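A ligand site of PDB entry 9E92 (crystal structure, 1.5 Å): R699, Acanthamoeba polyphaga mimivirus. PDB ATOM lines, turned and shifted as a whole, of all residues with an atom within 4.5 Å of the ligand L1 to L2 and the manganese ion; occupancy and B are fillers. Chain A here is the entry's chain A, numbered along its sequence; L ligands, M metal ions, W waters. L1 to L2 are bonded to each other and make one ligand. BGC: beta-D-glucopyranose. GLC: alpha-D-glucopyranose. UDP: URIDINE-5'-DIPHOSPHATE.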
ATOM      1  N   LEU A  56      -8.208  26.004  32.334  1.00  0.00           N
ATOM      2  CA  LEU A  56      -8.727  25.728  31.002  1.00  0.00           C
ATOM      3  C   LEU A  56      -7.669  25.941  29.907  1.00  0.00           C
ATOM      4  O   LEU A  56      -7.862  25.512  28.764  1.00  0.00           O
ATOM      5  CB  LEU A  56      -9.998  26.519  30.708  1.00  0.00           C
ATOM      6  CG  LEU A  56     -11.169  26.371  31.671  1.00  0.00           C
ATOM      7  CD1 LEU A  56     -12.371  27.170  31.196  1.00  0.00           C
ATOM      8  CD2 LEU A  56     -11.501  24.864  31.828  1.00  0.00           C
ATOM      9  N   ALA A  60      -9.345  20.054  30.288  1.00  0.00           N
ATOM     10  CA  ALA A  60     -10.796  20.139  30.278  1.00  0.00           C
ATOM     11  C   ALA A  60     -11.298  20.666  31.587  1.00  0.00           C
ATOM     12  O   ALA A  60     -10.662  20.505  32.619  1.00  0.00           O
ATOM     13  CB  ALA A  60     -11.435  18.781  30.018  1.00  0.00           C
ATOM     14  N   GLY A  61     -12.491  21.263  31.558  1.00  0.00           N
ATOM     15  CA  GLY A  61     -13.113  21.888  32.703  1.00  0.00           C
ATOM     16  C   GLY A  61     -14.285  22.773  32.328  1.00  0.00           C
ATOM     17  O   GLY A  61     -14.804  22.691  31.200  1.00  0.00           O
ATOM     18  N   LYS A  65     -19.320  26.861  35.277  1.00  0.00           N
ATOM     19  CA  LYS A  65     -20.078  27.842  34.535  1.00  0.00           C
ATOM     20  C   LYS A  65     -21.566  27.424  34.424  1.00  0.00           C
ATOM     21  O   LYS A  65     -22.437  28.267  34.579  1.00  0.00           O
ATOM     22  CB  LYS A  65     -19.467  27.976  33.124  1.00  0.00           C
ATOM     23  CG  LYS A  65     -18.047  28.468  33.037  1.00  0.00           C
ATOM     24  CD  LYS A  65     -17.397  28.177  31.678  1.00  0.00           C
ATOM     25  CE  LYS A  65     -18.068  28.826  30.554  1.00  0.00           C
ATOM     26  NZ  LYS A  65     -17.750  28.387  29.168  1.00  0.00           N
ATOM     27  N   ASP A  86     -18.921  33.456  27.357  1.00  0.00           N
ATOM     28  CA  ASP A  86     -17.605  33.757  27.933  1.00  0.00           C
ATOM     29  C   ASP A  86     -17.428  35.276  28.014  1.00  0.00           C
ATOM     30  O   ASP A  86     -18.023  35.995  27.191  1.00  0.00           O
ATOM     31  CB  ASP A  86     -16.451  33.123  27.171  1.00  0.00           C
ATOM     32  CG  ASP A  86     -16.265  31.622  27.289  1.00  0.00           C
ATOM     33  OD1 ASP A  86     -17.194  31.001  27.951  1.00  0.00           O
ATOM     34  OD2 ASP A  86     -15.209  31.029  26.839  1.00  0.00           O
ATOM     35  N   ASP A  89     -12.361  36.542  27.255  1.00  0.00           N
ATOM     36  CA  ASP A  89     -11.749  36.533  25.938  1.00  0.00           C
ATOM     37  C   ASP A  89     -12.779  36.787  24.820  1.00  0.00           C
ATOM     38  O   ASP A  89     -12.701  36.149  23.756  1.00  0.00           O
ATOM     39  CB  ASP A  89     -11.069  35.174  25.708  1.00  0.00           C
ATOM     40  CG  ASP A  89     -11.984  33.946  25.840  1.00  0.00           C
ATOM     41  OD1 ASP A  89     -13.157  34.120  26.207  1.00  0.00           O
ATOM     42  OD2 ASP A  89     -11.490  32.841  25.474  1.00  0.00           O
ATOM     43  N   GLU A 117     -16.886  25.785  15.903  1.00  0.00           N
ATOM     44  CA  GLU A 117     -15.435  25.939  15.916  1.00  0.00           C
ATOM     45  C   GLU A 117     -14.795  24.856  15.051  1.00  0.00           C
ATOM     46  O   GLU A 117     -15.478  23.952  14.564  1.00  0.00           O
ATOM     47  CB  GLU A 117     -14.787  25.997  17.310  1.00  0.00           C
ATOM     48  CG  GLU A 117     -14.853  24.637  18.047  1.00  0.00           C
ATOM     49  CD  GLU A 117     -13.786  24.592  19.124  1.00  0.00           C
ATOM     50  OE1 GLU A 117     -12.600  24.467  18.691  1.00  0.00           O
ATOM     51  OE2 GLU A 117     -14.108  24.820  20.322  1.00  0.00           O
ATOM     52  N   TYR A 119     -12.328  22.671  15.851  1.00  0.00           N
ATOM     53  CA  TYR A 119     -11.810  21.459  16.496  1.00  0.00           C
ATOM     54  C   TYR A 119     -12.845  20.791  17.371  1.00  0.00           C
ATOM     55  O   TYR A 119     -13.713  21.424  17.975  1.00  0.00           O
ATOM     56  CB  TYR A 119     -10.615  21.862  17.345  1.00  0.00           C
ATOM     57  CG  TYR A 119      -9.516  22.414  16.473  1.00  0.00           C
ATOM     58  CD1 TYR A 119      -8.960  21.660  15.428  1.00  0.00           C
ATOM     59  CD2 TYR A 119      -9.134  23.732  16.611  1.00  0.00           C
ATOM     60  CE1 TYR A 119      -8.009  22.209  14.589  1.00  0.00           C
ATOM     61  CE2 TYR A 119      -8.177  24.291  15.779  1.00  0.00           C
ATOM     62  CZ  TYR A 119      -7.610  23.530  14.778  1.00  0.00           C
ATOM     63  OH  TYR A 119      -6.655  24.117  13.990  1.00  0.00           O
ATOM     64  N   TRP A 121     -13.416  19.114  20.595  1.00  0.00           N
ATOM     65  CA  TRP A 121     -12.769  19.263  21.890  1.00  0.00           C
ATOM     66  C   TRP A 121     -13.846  19.204  22.961  1.00  0.00           C
ATOM     67  O   TRP A 121     -14.930  19.791  22.798  1.00  0.00           O
ATOM     68  CB  TRP A 121     -12.012  20.600  21.998  1.00  0.00           C
ATOM     69  CG  TRP A 121     -11.686  21.027  23.401  1.00  0.00           C
ATOM     70  CD1 TRP A 121     -12.460  21.781  24.218  1.00  0.00           C
ATOM     71  CD2 TRP A 121     -10.548  20.640  24.193  1.00  0.00           C
ATOM     72  NE1 TRP A 121     -11.881  21.939  25.449  1.00  0.00           N
ATOM     73  CE2 TRP A 121     -10.700  21.253  25.463  1.00  0.00           C
ATOM     74  CE3 TRP A 121      -9.392  19.882  23.947  1.00  0.00           C
ATOM     75  CZ2 TRP A 121      -9.761  21.119  26.473  1.00  0.00           C
ATOM     76  CZ3 TRP A 121      -8.485  19.724  24.965  1.00  0.00           C
ATOM     77  CH2 TRP A 121      -8.667  20.339  26.203  1.00  0.00           C
ATOM     78  N   ASN A 141     -18.831  24.900  19.990  1.00  0.00           N
ATOM     79  CA  ASN A 141     -18.092  25.653  21.001  1.00  0.00           C
ATOM     80  C   ASN A 141     -19.092  26.225  22.010  1.00  0.00           C
ATOM     81  O   ASN A 141     -20.093  26.887  21.657  1.00  0.00           O
ATOM     82  CB  ASN A 141     -17.245  26.784  20.366  1.00  0.00           C
ATOM     83  CG  ASN A 141     -16.486  27.574  21.418  1.00  0.00           C
ATOM     84  OD1 ASN A 141     -17.091  28.486  21.989  1.00  0.00           O
ATOM     85  ND2 ASN A 141     -15.243  27.229  21.675  1.00  0.00           N
ATOM     86  N   SER A 142     -18.845  25.976  23.322  1.00  0.00           N
ATOM     87  CA  SER A 142     -19.782  26.338  24.371  1.00  0.00           C
ATOM     88  C   SER A 142     -19.512  27.712  25.005  1.00  0.00           C
ATOM     89  O   SER A 142     -20.208  28.093  25.932  1.00  0.00           O
ATOM     90  CB  SER A 142     -19.830  25.253  25.454  1.00  0.00           C
ATOM     91  OG  SER A 142     -18.538  25.179  26.079  1.00  0.00           O
ATOM     92  N   GLY A 143     -18.607  28.483  24.382  1.00  0.00           N
ATOM     93  CA  GLY A 143     -18.305  29.820  24.849  1.00  0.00           C
ATOM     94  C   GLY A 143     -19.296  30.903  24.435  1.00  0.00           C
ATOM     95  O   GLY A 143     -19.220  32.052  24.897  1.00  0.00           O
ATOM     96  N   ASP A 165     -16.471  19.038  32.046  1.00  0.00           N
ATOM     97  CA  ASP A 165     -16.265  19.904  30.881  1.00  0.00           C
ATOM     98  C   ASP A 165     -17.596  20.387  30.324  1.00  0.00           C
ATOM     99  O   ASP A 165     -18.457  19.580  29.945  1.00  0.00           O
ATOM    100  CB  ASP A 165     -15.450  19.186  29.813  1.00  0.00           C
ATOM    101  CG  ASP A 165     -14.957  20.206  28.787  1.00  0.00           C
ATOM    102  OD1 ASP A 165     -15.793  20.555  27.930  1.00  0.00           O
ATOM    103  OD2 ASP A 165     -13.789  20.622  28.913  1.00  0.00           O
ATOM    104  N   ASP A 166     -17.789  21.723  30.254  1.00  0.00           N
ATOM    105  CA  ASP A 166     -19.067  22.267  29.782  1.00  0.00           C
ATOM    106  C   ASP A 166     -19.232  22.063  28.280  1.00  0.00           C
ATOM    107  O   ASP A 166     -20.364  21.978  27.774  1.00  0.00           O
ATOM    108  CB  ASP A 166     -19.217  23.723  30.176  1.00  0.00           C
ATOM    109  CG  ASP A 166     -18.240  24.730  29.567  1.00  0.00           C
ATOM    110  OD1 ASP A 166     -17.028  24.602  29.843  1.00  0.00           O
ATOM    111  OD2 ASP A 166     -18.710  25.646  28.852  1.00  0.00           O
ATOM    112  N   GLN A 167     -18.142  22.143  27.526  1.00  0.00           N
ATOM    113  CA  GLN A 167     -18.216  21.973  26.075  1.00  0.00           C
ATOM    114  C   GLN A 167     -18.613  20.535  25.764  1.00  0.00           C
ATOM    115  O   GLN A 167     -19.457  20.341  24.880  1.00  0.00           O
ATOM    116  CB  GLN A 167     -16.916  22.404  25.382  1.00  0.00           C
ATOM    117  CG  GLN A 167     -16.989  22.249  23.854  1.00  0.00           C
ATOM    118  CD  GLN A 167     -16.118  23.272  23.146  1.00  0.00           C
ATOM    119  OE1 GLN A 167     -16.275  24.476  23.344  1.00  0.00           O
ATOM    120  NE2 GLN A 167     -15.201  22.771  22.367  1.00  0.00           N
ATOM    121  N   TYR A 193      -9.906  30.897  17.064  1.00  0.00           N
ATOM    122  CA  TYR A 193      -8.690  30.096  17.049  1.00  0.00           C
ATOM    123  C   TYR A 193      -8.495  29.339  15.728  1.00  0.00           C
ATOM    124  O   TYR A 193      -9.435  28.668  15.237  1.00  0.00           O
ATOM    125  CB  TYR A 193      -8.704  29.121  18.235  1.00  0.00           C
ATOM    126  CG  TYR A 193      -7.389  28.380  18.378  1.00  0.00           C
ATOM    127  CD1 TYR A 193      -6.165  29.022  18.312  1.00  0.00           C
ATOM    128  CD2 TYR A 193      -7.385  27.004  18.598  1.00  0.00           C
ATOM    129  CE1 TYR A 193      -4.959  28.348  18.427  1.00  0.00           C
ATOM    130  CE2 TYR A 193      -6.183  26.322  18.767  1.00  0.00           C
ATOM    131  CZ  TYR A 193      -4.976  26.987  18.683  1.00  0.00           C
ATOM    132  OH  TYR A 193      -3.770  26.327  18.846  1.00  0.00           O
ATOM    133  N   HIS A 219     -14.825  35.935  19.753  1.00  0.00           N
ATOM    134  CA  HIS A 219     -14.345  35.081  20.824  1.00  0.00           C
ATOM    135  C   HIS A 219     -12.925  34.590  20.507  1.00  0.00           C
ATOM    136  O   HIS A 219     -12.703  33.727  19.644  1.00  0.00           O
ATOM    137  CB  HIS A 219     -15.330  33.903  20.984  1.00  0.00           C
ATOM    138  CG  HIS A 219     -14.989  32.977  22.099  1.00  0.00           C
ATOM    139  ND1 HIS A 219     -15.537  31.712  22.218  1.00  0.00           N
ATOM    140  CD2 HIS A 219     -14.151  33.133  23.234  1.00  0.00           C
ATOM    141  CE1 HIS A 219     -15.090  31.157  23.359  1.00  0.00           C
ATOM    142  NE2 HIS A 219     -14.226  31.975  24.005  1.00  0.00           N
ATOM    143  N   ASN A 221     -10.948  32.314  21.568  1.00  0.00           N
ATOM    144  CA  ASN A 221     -10.927  31.057  22.314  1.00  0.00           C
ATOM    145  C   ASN A 221      -9.522  30.458  22.290  1.00  0.00           C
ATOM    146  O   ASN A 221      -8.714  30.619  21.359  1.00  0.00           O
ATOM    147  CB  ASN A 221     -11.987  30.086  21.820  1.00  0.00           C
ATOM    148  CG  ASN A 221     -11.786  29.600  20.407  1.00  0.00           C
ATOM    149  OD1 ASN A 221     -11.643  30.429  19.472  1.00  0.00           O
ATOM    150  ND2 ASN A 221     -11.688  28.290  20.179  1.00  0.00           N
ATOM    151  N   GLY A 222      -9.157  29.800  23.399  1.00  0.00           N
ATOM    152  CA  GLY A 222      -7.853  29.183  23.485  1.00  0.00           C
ATOM    153  C   GLY A 222      -6.731  30.213  23.294  1.00  0.00           C
ATOM    154  O   GLY A 222      -6.852  31.342  23.775  1.00  0.00           O
ATOM    155  N   PRO A 223      -5.641  29.897  22.584  1.00  0.00           N
ATOM    156  CA  PRO A 223      -4.579  30.858  22.311  1.00  0.00           C
ATOM    157  C   PRO A 223      -4.985  32.092  21.512  1.00  0.00           C
ATOM    158  O   PRO A 223      -4.204  33.044  21.462  1.00  0.00           O
ATOM    159  CB  PRO A 223      -3.500  30.025  21.566  1.00  0.00           C
ATOM    160  CG  PRO A 223      -3.845  28.604  21.969  1.00  0.00           C
ATOM    161  CD  PRO A 223      -5.312  28.530  22.131  1.00  0.00           C
HETATM  162  C2  BGC L   1     -11.301  26.079  24.406  1.00  0.00           C
HETATM  163  C3  BGC L   1     -11.599  25.380  23.051  1.00  0.00           C
HETATM  164  C4  BGC L   1     -10.335  24.865  22.367  1.00  0.00           C
HETATM  165  C5  BGC L   1      -9.573  24.026  23.411  1.00  0.00           C
HETATM  166  C6  BGC L   1      -8.239  23.541  22.926  1.00  0.00           C
HETATM  167  C1  BGC L   1     -10.519  25.154  25.350  1.00  0.00           C
HETATM  168  O1  BGC L   1     -10.259  25.728  26.627  1.00  0.00           O
HETATM  169  O2  BGC L   1     -12.480  26.537  25.085  1.00  0.00           O
HETATM  170  O3  BGC L   1     -12.281  26.267  22.160  1.00  0.00           O
HETATM  171  O4  BGC L   1     -10.664  24.075  21.197  1.00  0.00           O
HETATM  172  O5  BGC L   1      -9.342  24.813  24.615  1.00  0.00           O
HETATM  173  O6  BGC L   1      -7.451  24.653  22.506  1.00  0.00           O
HETATM  174  C1  GLC L   2     -13.841  25.902  24.984  1.00  0.00           C
HETATM  175  C2  GLC L   2     -14.804  27.016  25.269  1.00  0.00           C
HETATM  176  C3  GLC L   2     -14.912  27.405  26.740  1.00  0.00           C
HETATM  177  C4  GLC L   2     -15.216  26.151  27.542  1.00  0.00           C
HETATM  178  C5  GLC L   2     -14.100  25.128  27.270  1.00  0.00           C
HETATM  179  C6  GLC L   2     -14.322  23.822  28.034  1.00  0.00           C
HETATM  180  O2  GLC L   2     -14.422  28.141  24.421  1.00  0.00           O
HETATM  181  O3  GLC L   2     -15.974  28.322  26.980  1.00  0.00           O
HETATM  182  O4  GLC L   2     -15.355  26.455  28.913  1.00  0.00           O
HETATM  183  O5  GLC L   2     -14.017  24.799  25.886  1.00  0.00           O
HETATM  184  O6  GLC L   2     -13.237  22.927  27.881  1.00  0.00           O
HETATM  185  N1  UDP L   3     -14.162  31.995  33.760  1.00  0.00           N
HETATM  186  C2  UDP L   3     -14.613  32.673  34.878  1.00  0.00           C
HETATM  187  N3  UDP L   3     -13.670  32.799  35.884  1.00  0.00           N
HETATM  188  C4  UDP L   3     -12.390  32.288  35.866  1.00  0.00           C
HETATM  189  C5  UDP L   3     -12.014  31.561  34.691  1.00  0.00           C
HETATM  190  C6  UDP L   3     -12.918  31.406  33.692  1.00  0.00           C
HETATM  191  O2  UDP L   3     -15.715  33.190  34.913  1.00  0.00           O
HETATM  192  O4  UDP L   3     -11.631  32.512  36.836  1.00  0.00           O
HETATM  193  C1' UDP L   3     -15.175  31.929  32.632  1.00  0.00           C
HETATM  194  C2' UDP L   3     -15.073  33.163  31.702  1.00  0.00           C
HETATM  195  O2' UDP L   3     -16.336  33.555  31.161  1.00  0.00           O
HETATM  196  C3' UDP L   3     -14.135  32.661  30.632  1.00  0.00           C
HETATM  197  C4' UDP L   3     -14.677  31.235  30.454  1.00  0.00           C
HETATM  198  O4' UDP L   3     -14.857  30.824  31.839  1.00  0.00           O
HETATM  199  O3' UDP L   3     -14.189  33.503  29.476  1.00  0.00           O
HETATM  200  C5' UDP L   3     -13.857  30.241  29.708  1.00  0.00           C
HETATM  201  O5' UDP L   3     -12.467  30.355  29.994  1.00  0.00           O
HETATM  202  PA  UDP L   3     -11.583  31.111  28.875  1.00  0.00           P
HETATM  203  O1A UDP L   3     -10.416  31.754  29.570  1.00  0.00           O
HETATM  204  O2A UDP L   3     -12.523  31.929  28.069  1.00  0.00           O
HETATM  205  O3A UDP L   3     -11.060  29.973  27.955  1.00  0.00           O
HETATM  206  PB  UDP L   3     -11.311  29.233  26.591  1.00  0.00           P
HETATM  207  O1B UDP L   3     -10.026  29.339  25.963  1.00  0.00           O
HETATM  208  O2B UDP L   3     -12.573  29.800  25.883  1.00  0.00           O
HETATM  209  O3B UDP L   3     -11.537  27.889  27.304  1.00  0.00           O
HETATM  210 MN    MN M   1     -13.395  31.765  26.040  1.00  0.00          MN
HETATM  211  O   HOH W   1     -10.643  23.842  28.398  1.00  0.00           O
HETATM  212  O   HOH W   2      -7.925  28.085  26.981  1.00  0.00           O
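The side-chain carboxylate of Asp 86 sits at hydrogen-bond distance from an oxygen (O3) of GLC L2, at 3.1 Å. OD2 of Asp 165 sits at hydrogen-bond distance from O6 of GLC L2 (2.6 Å). The side-chain carboxylate (OD1) of Asp 166 sits at hydrogen-bond distance from an oxygen (O4) of GLC L2 (2.7 Å). The side-chain amino group (NZ) of Lys 65 is in hydrogen-bond range of an oxygen (O3) of GLC L2, at 2.8 Å. ND2 of Asn 221 is in hydrogen-bond range of O3 of BGC L1. The indole nitrogen (NE1) of Trp 121 lies within hydrogen-bond range of an oxygen (O6) of GLC L2 (3.0 Å). OE2 of Glu 117 sits at hydrogen-bond distance from O3 of BGC L1. The side-chain amide nitrogen (ND2) of Asn 141 sits at hydrogen-bond distance from an oxygen (O2) of GLC L2. The backbone carbonyl oxygen of Leu 56 lies within hydrogen-bond range of an oxygen (O1) of BGC L1 (3.2 Å). The side-chain amide oxygen of Gln 167 lies close to an oxygen (O5) of GLC L2, at 3.4 Å. O1B of UDP L3 sits at hydrogen-bond distance from N of Gly 222.
O1 of BGC L1 is in hydrogen-bond range of O3B of UDP L3.
O of Gly 143 is in hydrogen-bond range of N of Asp 86 (2.8 Å). OD1 of Asp 165 is in hydrogen-bond range of N of Gln 167 (2.9 Å). The backbone NH of Gly 61 sits at hydrogen-bond distance from the side-chain carboxylate of Asp 165 (3.0 Å). The side-chain carboxylate (OD2) of Asp 166 lies within salt-bridge range of the side-chain amino group (NZ) of Lys 65 (2.9 Å). The backbone carbonyl oxygen (O) of Gly 61 sits at hydrogen-bond distance from the backbone NH (N) of Asp 166, at 3.3 Å. The side-chain amide oxygen (OD1) of Asn 221 is in hydrogen-bond range of the backbone NH (N) of Tyr 193 (3.0 Å). The side-chain carboxylate (OE1) of Glu 117 lies within hydrogen-bond range of the backbone NH (N) of Tyr 119. OE1 of Gln 167 lies close to ND2 of Asn 141, 3.4 Å away.
O of Gly 61 touches C6 of GLC L2, at 3.4 Å. Ser 142 touches the ligand L1 to L2. CA of Gly 143 touches O3 of GLC L2, 3.5 Å away. Hydrophobic or aromatic side chains that line the ligand L1 to L2: Leu 56, Trp 121 and His 219. Within 4 Å of the ligand L1 to L2: Leu 56, Gly 61, Lys 65, Asp 86, Glu 117, Trp 121, Asn 141, Ser 142, Gly 143, Asp 165, Asp 166, Gln 167, His 219 and Asn 221. The nearest printed residue that does not touch the ligand L1 to L2 is Tyr 193 (4.3 Å).
Within 4 Å of the manganese ion: Asp 86, Asp 89 and His 219. The nearest printed residue that does not touch the manganese ion is Asn 221 (4.5 Å).
OD2 of Asp 86 binds the manganese ion (2.1 Å). An oxygen (O2B) of UDP L3 is bound to the manganese ion, at 2.1 Å. NE2 of His 219 is bound to the manganese ion (2.2 Å). The manganese ion is bound by O2A of UDP L3 (2.2 Å). The side-chain carboxylate (OD2) of Asp 89 is bound to the manganese ion, 2.3 Å away. The manganese ion is bound by OD1 of Asp 89 (2.4 Å).
Water W1 lies within hydrogen-bond range of an oxygen (O1) of BGC L1 (2.6 Å) and the backbone carbonyl oxygen of Leu 56 (3.3 Å). Water W2 lies within hydrogen-bond range of an oxygen (O1B) of UDP L3, the backbone carbonyl oxygen (O) of Leu 56 and an oxygen (O1) of BGC L1.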
